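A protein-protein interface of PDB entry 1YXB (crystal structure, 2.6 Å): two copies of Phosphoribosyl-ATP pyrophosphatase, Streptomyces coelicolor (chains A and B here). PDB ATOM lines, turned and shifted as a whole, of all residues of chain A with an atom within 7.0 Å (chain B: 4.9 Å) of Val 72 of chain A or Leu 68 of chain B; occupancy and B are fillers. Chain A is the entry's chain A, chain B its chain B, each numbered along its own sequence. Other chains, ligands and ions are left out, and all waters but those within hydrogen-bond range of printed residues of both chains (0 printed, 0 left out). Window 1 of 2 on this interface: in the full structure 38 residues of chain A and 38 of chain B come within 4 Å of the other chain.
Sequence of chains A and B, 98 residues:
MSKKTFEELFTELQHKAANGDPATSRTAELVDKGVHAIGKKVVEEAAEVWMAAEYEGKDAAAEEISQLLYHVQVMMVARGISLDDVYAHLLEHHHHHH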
ATOM      1  N   PHE A   6       3.012 -10.385 -29.128  1.00  0.00           N
ATOM      2  CA  PHE A   6       2.188 -10.796 -27.991  1.00  0.00           C
ATOM      3  C   PHE A   6       1.465 -12.082 -28.369  1.00  0.00           C
ATOM      4  O   PHE A   6       1.441 -13.039 -27.596  1.00  0.00           O
ATOM      5  CB  PHE A   6       1.164  -9.694 -27.674  1.00  0.00           C
ATOM      6  CG  PHE A   6       0.433  -9.862 -26.352  1.00  0.00           C
ATOM      7  CD1 PHE A   6       1.075  -9.602 -25.145  1.00  0.00           C
ATOM      8  CD2 PHE A   6      -0.918 -10.208 -26.325  1.00  0.00           C
ATOM      9  CE1 PHE A   6       0.381  -9.676 -23.935  1.00  0.00           C
ATOM     10  CE2 PHE A   6      -1.619 -10.284 -25.119  1.00  0.00           C
ATOM     11  CZ  PHE A   6      -0.968 -10.018 -23.925  1.00  0.00           C
ATOM     12  N   PHE A  10       1.891 -16.010 -26.748  1.00  0.00           N
ATOM     13  CA  PHE A  10       0.689 -16.592 -26.158  1.00  0.00           C
ATOM     14  C   PHE A  10       0.424 -18.011 -26.652  1.00  0.00           C
ATOM     15  O   PHE A  10       0.007 -18.867 -25.875  1.00  0.00           O
ATOM     16  CB  PHE A  10      -0.539 -15.717 -26.422  1.00  0.00           C
ATOM     17  CG  PHE A  10      -1.798 -16.248 -25.798  1.00  0.00           C
ATOM     18  CD1 PHE A  10      -1.912 -16.344 -24.419  1.00  0.00           C
ATOM     19  CD2 PHE A  10      -2.854 -16.693 -26.591  1.00  0.00           C
ATOM     20  CE1 PHE A  10      -3.054 -16.879 -23.840  1.00  0.00           C
ATOM     21  CE2 PHE A  10      -3.998 -17.228 -26.025  1.00  0.00           C
ATOM     22  CZ  PHE A  10      -4.101 -17.325 -24.646  1.00  0.00           C
ATOM     23  N   ILE A  38      -2.825 -18.292  -9.649  1.00  0.00           N
ATOM     24  CA  ILE A  38      -2.512 -17.348 -10.702  1.00  0.00           C
ATOM     25  C   ILE A  38      -3.018 -15.981 -10.314  1.00  0.00           C
ATOM     26  O   ILE A  38      -2.361 -14.988 -10.572  1.00  0.00           O
ATOM     27  CB  ILE A  38      -3.118 -17.777 -12.027  1.00  0.00           C
ATOM     28  CG1 ILE A  38      -2.531 -19.126 -12.432  1.00  0.00           C
ATOM     29  CG2 ILE A  38      -2.822 -16.738 -13.095  1.00  0.00           C
ATOM     30  CD1 ILE A  38      -3.275 -19.835 -13.548  1.00  0.00           C
ATOM     31  N   VAL A  42      -1.275 -12.234 -10.169  1.00  0.00           N
ATOM     32  CA  VAL A  42      -1.762 -11.125 -10.947  1.00  0.00           C
ATOM     33  C   VAL A  42      -1.919  -9.904 -10.086  1.00  0.00           C
ATOM     34  O   VAL A  42      -1.523  -8.804 -10.460  1.00  0.00           O
ATOM     35  CB  VAL A  42      -3.077 -11.474 -11.615  1.00  0.00           C
ATOM     36  CG1 VAL A  42      -3.738 -10.214 -12.188  1.00  0.00           C
ATOM     37  CG2 VAL A  42      -2.816 -12.487 -12.737  1.00  0.00           C
ATOM     38  N   ALA A  46       0.449  -6.481 -10.144  1.00  0.00           N
ATOM     39  CA  ALA A  46      -0.187  -5.213 -10.449  1.00  0.00           C
ATOM     40  C   ALA A  46       0.325  -4.151  -9.462  1.00  0.00           C
ATOM     41  O   ALA A  46       0.582  -3.005  -9.857  1.00  0.00           O
ATOM     42  CB  ALA A  46      -1.678  -5.360 -10.341  1.00  0.00           C
ATOM     43  N   SER A  66       6.144  -6.859 -17.707  1.00  0.00           N
ATOM     44  CA  SER A  66       6.272  -8.114 -18.447  1.00  0.00           C
ATOM     45  C   SER A  66       5.800  -9.270 -17.577  1.00  0.00           C
ATOM     46  O   SER A  66       5.122 -10.180 -18.049  1.00  0.00           O
ATOM     47  CB  SER A  66       7.712  -8.346 -18.909  1.00  0.00           C
ATOM     48  OG  SER A  66       8.539  -8.768 -17.844  1.00  0.00           O
ATOM     49  N   GLN A  67       6.140  -9.218 -16.295  1.00  0.00           N
ATOM     50  CA  GLN A  67       5.710 -10.251 -15.370  1.00  0.00           C
ATOM     51  C   GLN A  67       4.184 -10.249 -15.247  1.00  0.00           C
ATOM     52  O   GLN A  67       3.557 -11.307 -15.223  1.00  0.00           O
ATOM     53  CB  GLN A  67       6.360 -10.036 -14.011  1.00  0.00           C
ATOM     54  CG  GLN A  67       7.789 -10.531 -13.932  1.00  0.00           C
ATOM     55  CD  GLN A  67       7.873 -12.052 -13.911  1.00  0.00           C
ATOM     56  OE1 GLN A  67       7.428 -12.703 -12.951  1.00  0.00           O
ATOM     57  NE2 GLN A  67       8.434 -12.630 -14.975  1.00  0.00           N
ATOM     58  N   LEU A  68       3.581  -9.063 -15.238  1.00  0.00           N
ATOM     59  CA  LEU A  68       2.125  -8.948 -15.123  1.00  0.00           C
ATOM     60  C   LEU A  68       1.423  -9.495 -16.356  1.00  0.00           C
ATOM     61  O   LEU A  68       0.406 -10.178 -16.254  1.00  0.00           O
ATOM     62  CB  LEU A  68       1.719  -7.493 -14.889  1.00  0.00           C
ATOM     63  CG  LEU A  68       0.224  -7.169 -14.845  1.00  0.00           C
ATOM     64  CD1 LEU A  68      -0.452  -8.011 -13.804  1.00  0.00           C
ATOM     65  CD2 LEU A  68       0.011  -5.692 -14.558  1.00  0.00           C
ATOM     66  N   LEU A  69       1.983  -9.207 -17.522  1.00  0.00           N
ATOM     67  CA  LEU A  69       1.407  -9.677 -18.765  1.00  0.00           C
ATOM     68  C   LEU A  69       1.521 -11.179 -18.854  1.00  0.00           C
ATOM     69  O   LEU A  69       0.577 -11.849 -19.246  1.00  0.00           O
ATOM     70  CB  LEU A  69       2.080  -9.020 -19.964  1.00  0.00           C
ATOM     71  CG  LEU A  69       1.883  -7.515 -20.081  1.00  0.00           C
ATOM     72  CD1 LEU A  69       2.553  -6.999 -21.340  1.00  0.00           C
ATOM     73  CD2 LEU A  69       0.429  -7.208 -20.090  1.00  0.00           C
ATOM     74  N   TYR A  70       2.667 -11.706 -18.438  1.00  0.00           N
ATOM     75  CA  TYR A  70       2.888 -13.144 -18.447  1.00  0.00           C
ATOM     76  C   TYR A  70       1.811 -13.865 -17.640  1.00  0.00           C
ATOM     77  O   TYR A  70       1.167 -14.794 -18.141  1.00  0.00           O
ATOM     78  CB  TYR A  70       4.270 -13.487 -17.905  1.00  0.00           C
ATOM     79  CG  TYR A  70       4.458 -14.963 -17.673  1.00  0.00           C
ATOM     80  CD1 TYR A  70       4.500 -15.860 -18.734  1.00  0.00           C
ATOM     81  CD2 TYR A  70       4.525 -15.471 -16.383  1.00  0.00           C
ATOM     82  CE1 TYR A  70       4.597 -17.226 -18.507  1.00  0.00           C
ATOM     83  CE2 TYR A  70       4.623 -16.830 -16.148  1.00  0.00           C
ATOM     84  CZ  TYR A  70       4.652 -17.707 -17.211  1.00  0.00           C
ATOM     85  OH  TYR A  70       4.692 -19.065 -16.962  1.00  0.00           O
ATOM     86  N   HIS A  71       1.557 -13.386 -16.424  1.00  0.00           N
ATOM     87  CA  HIS A  71       0.559 -14.005 -15.574  1.00  0.00           C
ATOM     88  C   HIS A  71      -0.859 -13.783 -16.060  1.00  0.00           C
ATOM     89  O   HIS A  71      -1.721 -14.619 -15.818  1.00  0.00           O
ATOM     90  CB  HIS A  71       0.738 -13.575 -14.124  1.00  0.00           C
ATOM     91  CG  HIS A  71       2.014 -14.063 -13.510  1.00  0.00           C
ATOM     92  ND1 HIS A  71       2.173 -15.355 -13.069  1.00  0.00           N
ATOM     93  CD2 HIS A  71       3.190 -13.435 -13.286  1.00  0.00           C
ATOM     94  CE1 HIS A  71       3.403 -15.506 -12.598  1.00  0.00           C
ATOM     95  NE2 HIS A  71       4.035 -14.361 -12.719  1.00  0.00           N
ATOM     96  N   VAL A  72      -1.120 -12.653 -16.721  1.00  0.00           N
ATOM     97  CA  VAL A  72      -2.458 -12.403 -17.264  1.00  0.00           C
ATOM     98  C   VAL A  72      -2.687 -13.439 -18.354  1.00  0.00           C
ATOM     99  O   VAL A  72      -3.767 -14.039 -18.421  1.00  0.00           O
ATOM    100  CB  VAL A  72      -2.618 -10.984 -17.869  1.00  0.00           C
ATOM    101  CG1 VAL A  72      -3.893 -10.898 -18.682  1.00  0.00           C
ATOM    102  CG2 VAL A  72      -2.672  -9.952 -16.776  1.00  0.00           C
ATOM    103  N   GLN A  73      -1.649 -13.664 -19.176  1.00  0.00           N
ATOM    104  CA  GLN A  73      -1.688 -14.655 -20.260  1.00  0.00           C
ATOM    105  C   GLN A  73      -1.904 -16.068 -19.728  1.00  0.00           C
ATOM    106  O   GLN A  73      -2.655 -16.848 -20.310  1.00  0.00           O
ATOM    107  CB  GLN A  73      -0.407 -14.628 -21.100  1.00  0.00           C
ATOM    108  CG  GLN A  73      -0.352 -13.487 -22.092  1.00  0.00           C
ATOM    109  CD  GLN A  73       0.760 -13.619 -23.115  1.00  0.00           C
ATOM    110  OE1 GLN A  73       0.705 -12.994 -24.169  1.00  0.00           O
ATOM    111  NE2 GLN A  73       1.768 -14.432 -22.817  1.00  0.00           N
ATOM    112  N   VAL A  74      -1.218 -16.398 -18.638  1.00  0.00           N
ATOM    113  CA  VAL A  74      -1.356 -17.702 -18.018  1.00  0.00           C
ATOM    114  C   VAL A  74      -2.808 -17.848 -17.574  1.00  0.00           C
ATOM    115  O   VAL A  74      -3.424 -18.895 -17.796  1.00  0.00           O
ATOM    116  CB  VAL A  74      -0.400 -17.849 -16.816  1.00  0.00           C
ATOM    117  CG1 VAL A  74      -0.661 -19.127 -16.086  1.00  0.00           C
ATOM    118  CG2 VAL A  74       1.016 -17.839 -17.276  1.00  0.00           C
ATOM    119  N   MET A  75      -3.372 -16.784 -17.002  1.00  0.00           N
ATOM    120  CA  MET A  75      -4.760 -16.798 -16.545  1.00  0.00           C
ATOM    121  C   MET A  75      -5.681 -17.075 -17.743  1.00  0.00           C
ATOM    122  O   MET A  75      -6.653 -17.807 -17.634  1.00  0.00           O
ATOM    123  CB  MET A  75      -5.099 -15.459 -15.877  1.00  0.00           C
ATOM    124  CG  MET A  75      -6.516 -15.341 -15.345  1.00  0.00           C
ATOM    125  SD  MET A  75      -6.608 -16.582 -13.846  1.00  0.00           S
ATOM    126  CE  MET A  75      -6.546 -15.381 -12.274  1.00  0.00           C
ATOM    127  N   MET A  76      -5.376 -16.475 -18.882  1.00  0.00           N
ATOM    128  CA  MET A  76      -6.166 -16.706 -20.085  1.00  0.00           C
ATOM    129  C   MET A  76      -6.112 -18.176 -20.492  1.00  0.00           C
ATOM    130  O   MET A  76      -7.125 -18.765 -20.868  1.00  0.00           O
ATOM    131  CB  MET A  76      -5.646 -15.851 -21.213  1.00  0.00           C
ATOM    132  CG  MET A  76      -5.867 -14.418 -20.956  1.00  0.00           C
ATOM    133  SD  MET A  76      -5.141 -13.385 -22.454  1.00  0.00           S
ATOM    134  CE  MET A  76      -3.603 -12.463 -21.694  1.00  0.00           C
ATOM    135  N   VAL A  77      -4.922 -18.758 -20.409  1.00  0.00           N
ATOM    136  CA  VAL A  77      -4.736 -20.158 -20.737  1.00  0.00           C
ATOM    137  C   VAL A  77      -5.514 -21.046 -19.781  1.00  0.00           C
ATOM    138  O   VAL A  77      -6.204 -21.964 -20.214  1.00  0.00           O
ATOM    139  CB  VAL A  77      -3.245 -20.549 -20.718  1.00  0.00           C
ATOM    140  CG1 VAL A  77      -3.082 -22.065 -20.773  1.00  0.00           C
ATOM    141  CG2 VAL A  77      -2.538 -19.908 -21.910  1.00  0.00           C
ATOM    142  N   ALA A  78      -5.446 -20.732 -18.494  1.00  0.00           N
ATOM    143  CA  ALA A  78      -6.127 -21.512 -17.467  1.00  0.00           C
ATOM    144  C   ALA A  78      -7.649 -21.512 -17.563  1.00  0.00           C
ATOM    145  O   ALA A  78      -8.307 -22.455 -17.107  1.00  0.00           O
ATOM    146  CB  ALA A  78      -5.694 -21.032 -16.098  1.00  0.00           C
ATOM    147  N   VAL A  86     -10.349 -11.473 -26.030  1.00  0.00           N
ATOM    148  CA  VAL A  86      -9.887 -10.267 -25.358  1.00  0.00           C
ATOM    149  C   VAL A  86      -9.819  -9.080 -26.309  1.00  0.00           C
ATOM    150  O   VAL A  86     -10.303  -7.994 -25.983  1.00  0.00           O
ATOM    151  CB  VAL A  86      -8.499 -10.493 -24.702  1.00  0.00           C
ATOM    152  CG1 VAL A  86      -7.899  -9.176 -24.218  1.00  0.00           C
ATOM    153  CG2 VAL A  86      -8.630 -11.451 -23.556  1.00  0.00           C
ATOM    154  N   VAL B  42      -4.896  -0.036 -12.421  1.00  0.00           N
ATOM    155  CA  VAL B  42      -4.225  -1.311 -12.654  1.00  0.00           C
ATOM    156  C   VAL B  42      -4.462  -2.281 -11.497  1.00  0.00           C
ATOM    157  O   VAL B  42      -4.824  -3.424 -11.690  1.00  0.00           O
ATOM    158  CB  VAL B  42      -2.699  -1.129 -12.893  1.00  0.00           C
ATOM    159  CG1 VAL B  42      -1.984  -2.465 -12.821  1.00  0.00           C
ATOM    160  CG2 VAL B  42      -2.440  -0.507 -14.289  1.00  0.00           C
ATOM    161  N   GLU B  45      -8.275  -3.307 -11.385  1.00  0.00           N
ATOM    162  CA  GLU B  45      -8.594  -4.224 -12.454  1.00  0.00           C
ATOM    163  C   GLU B  45      -7.984  -5.601 -12.220  1.00  0.00           C
ATOM    164  O   GLU B  45      -8.592  -6.591 -12.583  1.00  0.00           O
ATOM    165  CB  GLU B  45      -8.118  -3.682 -13.793  1.00  0.00           C
ATOM    166  CG  GLU B  45      -8.865  -2.457 -14.287  1.00  0.00           C
ATOM    167  CD  GLU B  45     -10.339  -2.708 -14.517  1.00  0.00           C
ATOM    168  OE1 GLU B  45     -10.740  -3.878 -14.760  1.00  0.00           O
ATOM    169  OE2 GLU B  45     -11.102  -1.719 -14.451  1.00  0.00           O
ATOM    170  N   ALA B  46      -6.785  -5.653 -11.633  1.00  0.00           N
ATOM    171  CA  ALA B  46      -6.111  -6.912 -11.329  1.00  0.00           C
ATOM    172  C   ALA B  46      -7.004  -7.755 -10.411  1.00  0.00           C
ATOM    173  O   ALA B  46      -7.207  -8.943 -10.649  1.00  0.00           O
ATOM    174  CB  ALA B  46      -4.770  -6.643 -10.669  1.00  0.00           C
ATOM    175  N   VAL B  49     -10.014  -8.952 -12.354  1.00  0.00           N
ATOM    176  CA  VAL B  49      -9.632 -10.062 -13.202  1.00  0.00           C
ATOM    177  C   VAL B  49      -9.655 -11.343 -12.363  1.00  0.00           C
ATOM    178  O   VAL B  49     -10.256 -12.333 -12.778  1.00  0.00           O
ATOM    179  CB  VAL B  49      -8.238  -9.826 -13.812  1.00  0.00           C
ATOM    180  CG1 VAL B  49      -7.626 -11.102 -14.306  1.00  0.00           C
ATOM    181  CG2 VAL B  49      -8.357  -8.880 -14.939  1.00  0.00           C
ATOM    182  N   GLU B  64     -12.741  -8.160 -18.342  1.00  0.00           N
ATOM    183  CA  GLU B  64     -11.928  -7.604 -17.271  1.00  0.00           C
ATOM    184  C   GLU B  64     -10.452  -7.615 -17.616  1.00  0.00           C
ATOM    185  O   GLU B  64      -9.730  -6.697 -17.250  1.00  0.00           O
ATOM    186  CB  GLU B  64     -12.153  -8.342 -15.959  1.00  0.00           C
ATOM    187  CG  GLU B  64     -13.568  -8.241 -15.414  1.00  0.00           C
ATOM    188  CD  GLU B  64     -14.016  -6.827 -15.135  1.00  0.00           C
ATOM    189  OE1 GLU B  64     -13.163  -5.939 -14.919  1.00  0.00           O
ATOM    190  OE2 GLU B  64     -15.245  -6.607 -15.124  1.00  0.00           O
ATOM    191  N   ILE B  65     -10.005  -8.667 -18.296  1.00  0.00           N
ATOM    192  CA  ILE B  65      -8.618  -8.782 -18.723  1.00  0.00           C
ATOM    193  C   ILE B  65      -8.290  -7.696 -19.744  1.00  0.00           C
ATOM    194  O   ILE B  65      -7.205  -7.133 -19.722  1.00  0.00           O
ATOM    195  CB  ILE B  65      -8.318 -10.174 -19.314  1.00  0.00           C
ATOM    196  CG1 ILE B  65      -8.233 -11.202 -18.197  1.00  0.00           C
ATOM    197  CG2 ILE B  65      -7.034 -10.162 -20.087  1.00  0.00           C
ATOM    198  CD1 ILE B  65      -7.923 -12.571 -18.666  1.00  0.00           C
ATOM    199  N   SER B  66      -9.241  -7.369 -20.612  1.00  0.00           N
ATOM    200  CA  SER B  66      -9.007  -6.335 -21.624  1.00  0.00           C
ATOM    201  C   SER B  66      -8.850  -4.967 -20.970  1.00  0.00           C
ATOM    202  O   SER B  66      -8.046  -4.158 -21.413  1.00  0.00           O
ATOM    203  CB  SER B  66     -10.116  -6.312 -22.680  1.00  0.00           C
ATOM    204  OG  SER B  66     -11.296  -5.729 -22.170  1.00  0.00           O
ATOM    205  N   GLN B  67      -9.607  -4.732 -19.900  1.00  0.00           N
ATOM    206  CA  GLN B  67      -9.524  -3.482 -19.158  1.00  0.00           C
ATOM    207  C   GLN B  67      -8.170  -3.382 -18.461  1.00  0.00           C
ATOM    208  O   GLN B  67      -7.582  -2.315 -18.390  1.00  0.00           O
ATOM    209  CB  GLN B  67     -10.647  -3.393 -18.124  1.00  0.00           C
ATOM    210  CG  GLN B  67     -11.997  -2.922 -18.667  1.00  0.00           C
ATOM    211  CD  GLN B  67     -11.996  -1.443 -19.056  1.00  0.00           C
ATOM    212  OE1 GLN B  67     -11.953  -0.560 -18.191  1.00  0.00           O
ATOM    213  NE2 GLN B  67     -12.060  -1.169 -20.361  1.00  0.00           N
ATOM    214  N   LEU B  68      -7.663  -4.507 -17.972  1.00  0.00           N
ATOM    215  CA  LEU B  68      -6.386  -4.513 -17.289  1.00  0.00           C
ATOM    216  C   LEU B  68      -5.271  -4.226 -18.272  1.00  0.00           C
ATOM    217  O   LEU B  68      -4.401  -3.399 -17.990  1.00  0.00           O
ATOM    218  CB  LEU B  68      -6.154  -5.847 -16.571  1.00  0.00           C
ATOM    219  CG  LEU B  68      -4.777  -6.097 -15.922  1.00  0.00           C
ATOM    220  CD1 LEU B  68      -4.457  -5.026 -14.880  1.00  0.00           C
ATOM    221  CD2 LEU B  68      -4.761  -7.487 -15.297  1.00  0.00           C
ATOM    222  N   LEU B  69      -5.295  -4.910 -19.418  1.00  0.00           N
ATOM    223  CA  LEU B  69      -4.282  -4.711 -20.441  1.00  0.00           C
ATOM    224  C   LEU B  69      -4.283  -3.259 -20.916  1.00  0.00           C
ATOM    225  O   LEU B  69      -3.225  -2.645 -21.043  1.00  0.00           O
ATOM    226  CB  LEU B  69      -4.501  -5.672 -21.604  1.00  0.00           C
ATOM    227  CG  LEU B  69      -4.362  -7.173 -21.304  1.00  0.00           C
ATOM    228  CD1 LEU B  69      -4.613  -7.950 -22.570  1.00  0.00           C
ATOM    229  CD2 LEU B  69      -2.982  -7.498 -20.756  1.00  0.00           C
ATOM    230  N   TYR B  70      -5.471  -2.703 -21.136  1.00  0.00           N
ATOM    231  CA  TYR B  70      -5.594  -1.325 -21.560  1.00  0.00           C
ATOM    232  C   TYR B  70      -4.877  -0.399 -20.583  1.00  0.00           C
ATOM    233  O   TYR B  70      -4.054   0.426 -21.002  1.00  0.00           O
ATOM    234  CB  TYR B  70      -7.068  -0.922 -21.696  1.00  0.00           C
ATOM    235  CG  TYR B  70      -7.272   0.569 -21.885  1.00  0.00           C
ATOM    236  CD1 TYR B  70      -6.855   1.220 -23.048  1.00  0.00           C
ATOM    237  CD2 TYR B  70      -7.812   1.338 -20.864  1.00  0.00           C
ATOM    238  CE1 TYR B  70      -6.969   2.610 -23.176  1.00  0.00           C
ATOM    239  CE2 TYR B  70      -7.929   2.712 -20.982  1.00  0.00           C
ATOM    240  CZ  TYR B  70      -7.501   3.346 -22.128  1.00  0.00           C
ATOM    241  OH  TYR B  70      -7.558   4.715 -22.175  1.00  0.00           O
ATOM    242  N   HIS B  71      -5.166  -0.538 -19.288  1.00  0.00           N
ATOM    243  CA  HIS B  71      -4.518   0.313 -18.288  1.00  0.00           C
ATOM    244  C   HIS B  71      -3.029   0.055 -18.142  1.00  0.00           C
ATOM    245  O   HIS B  71      -2.291   0.957 -17.773  1.00  0.00           O
ATOM    246  CB  HIS B  71      -5.225   0.263 -16.931  1.00  0.00           C
ATOM    247  CG  HIS B  71      -6.618   0.798 -16.963  1.00  0.00           C
ATOM    248  ND1 HIS B  71      -6.901   2.155 -16.990  1.00  0.00           N
ATOM    249  CD2 HIS B  71      -7.817   0.172 -17.014  1.00  0.00           C
ATOM    250  CE1 HIS B  71      -8.202   2.331 -17.060  1.00  0.00           C
ATOM    251  NE2 HIS B  71      -8.786   1.144 -17.077  1.00  0.00           N
ATOM    252  N   VAL B  72      -2.586  -1.171 -18.413  1.00  0.00           N
ATOM    253  CA  VAL B  72      -1.165  -1.488 -18.351  1.00  0.00           C
ATOM    254  C   VAL B  72      -0.521  -0.737 -19.494  1.00  0.00           C
ATOM    255  O   VAL B  72       0.490  -0.083 -19.282  1.00  0.00           O
ATOM    256  CB  VAL B  72      -0.893  -3.008 -18.482  1.00  0.00           C
ATOM    257  CG1 VAL B  72       0.562  -3.268 -18.815  1.00  0.00           C
ATOM    258  CG2 VAL B  72      -1.239  -3.691 -17.192  1.00  0.00           C
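Hydrophobic or aromatic side chains of chain A within 4 Å of the printed part of chain B: Ala 46, Leu 68, Leu 69, Val 72, Met 76 and Val 86.
Among the printed residues, 10 pairs touch across the chains.
Among the printed residues, no Asp or Glu carboxylate lies within 4 Å of a Lys or Arg side-chain nitrogen of the other chain.
Among the printed residues, merely in contact across the chains: Val 42 of chain A with Ala 46 of chain B, Ala 46 of chain A with Val 42 of chain B, Ala 46 of chain A with Ala 46 of chain B, Leu 68 of chain A with Val 72 of chain B, Leu 69 of chain A with Leu 69 of chain B, Val 72 of chain A with Ile 65 of chain B, Val 72 of chain A with Leu 68 of chain B, Met 76 of chain A with Ile 65 of chain B, Val 86 of chain A with Ser 66 of chain B and Val 86 of chain A with Leu 69 of chain B.
Printed residues of chain B within 4 Å of Val 72 of chain A: Ile 65 (3.5 Å) and Leu 68 (3.6 Å).
Of chain A, only Val 72 (3.6 Å) comes within 4 Å of Leu 68 of chain B.
Of the printed residues of chain B, Val 86 of chain A touches Ser 66 and Leu 69.
Printed residues of chain A within 4 Å of Leu 69 of chain B: Leu 69 (3.5 Å) and Val 86 (3.9 Å).
Of the printed residues of chain A, Val 42 of chain B touches Ala 46 (3.8 Å).
Ala 78 of chain A touches none of the printed residues of chain B.
The nearest residue of chain A that does not touch Leu 68 of chain B is Val 42 of chain A (4.3 Å).
Val 42 of chain A touches Ala 46 of chain B, and with the chains exchanged Ala 46 of chain A touches Val 42 of chain B.
Ala 46 of chain A touches its own counterpart, Ala 46 of chain B.
Leu 68 of chain A touches Val 72 of chain B, and with the chains exchanged Val 72 of chain A touches Leu 68 of chain B.
Leu 69 of chain B touches its own counterpart, Leu 69 of chain A.
Positions printed for both chains: 42, 46, 66, 67, 68, 69, 70, 71 and 72.
Of the 10 pairs that touch across the chains among the printed residues, 6 have their exchanged pair printed and touching as well.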
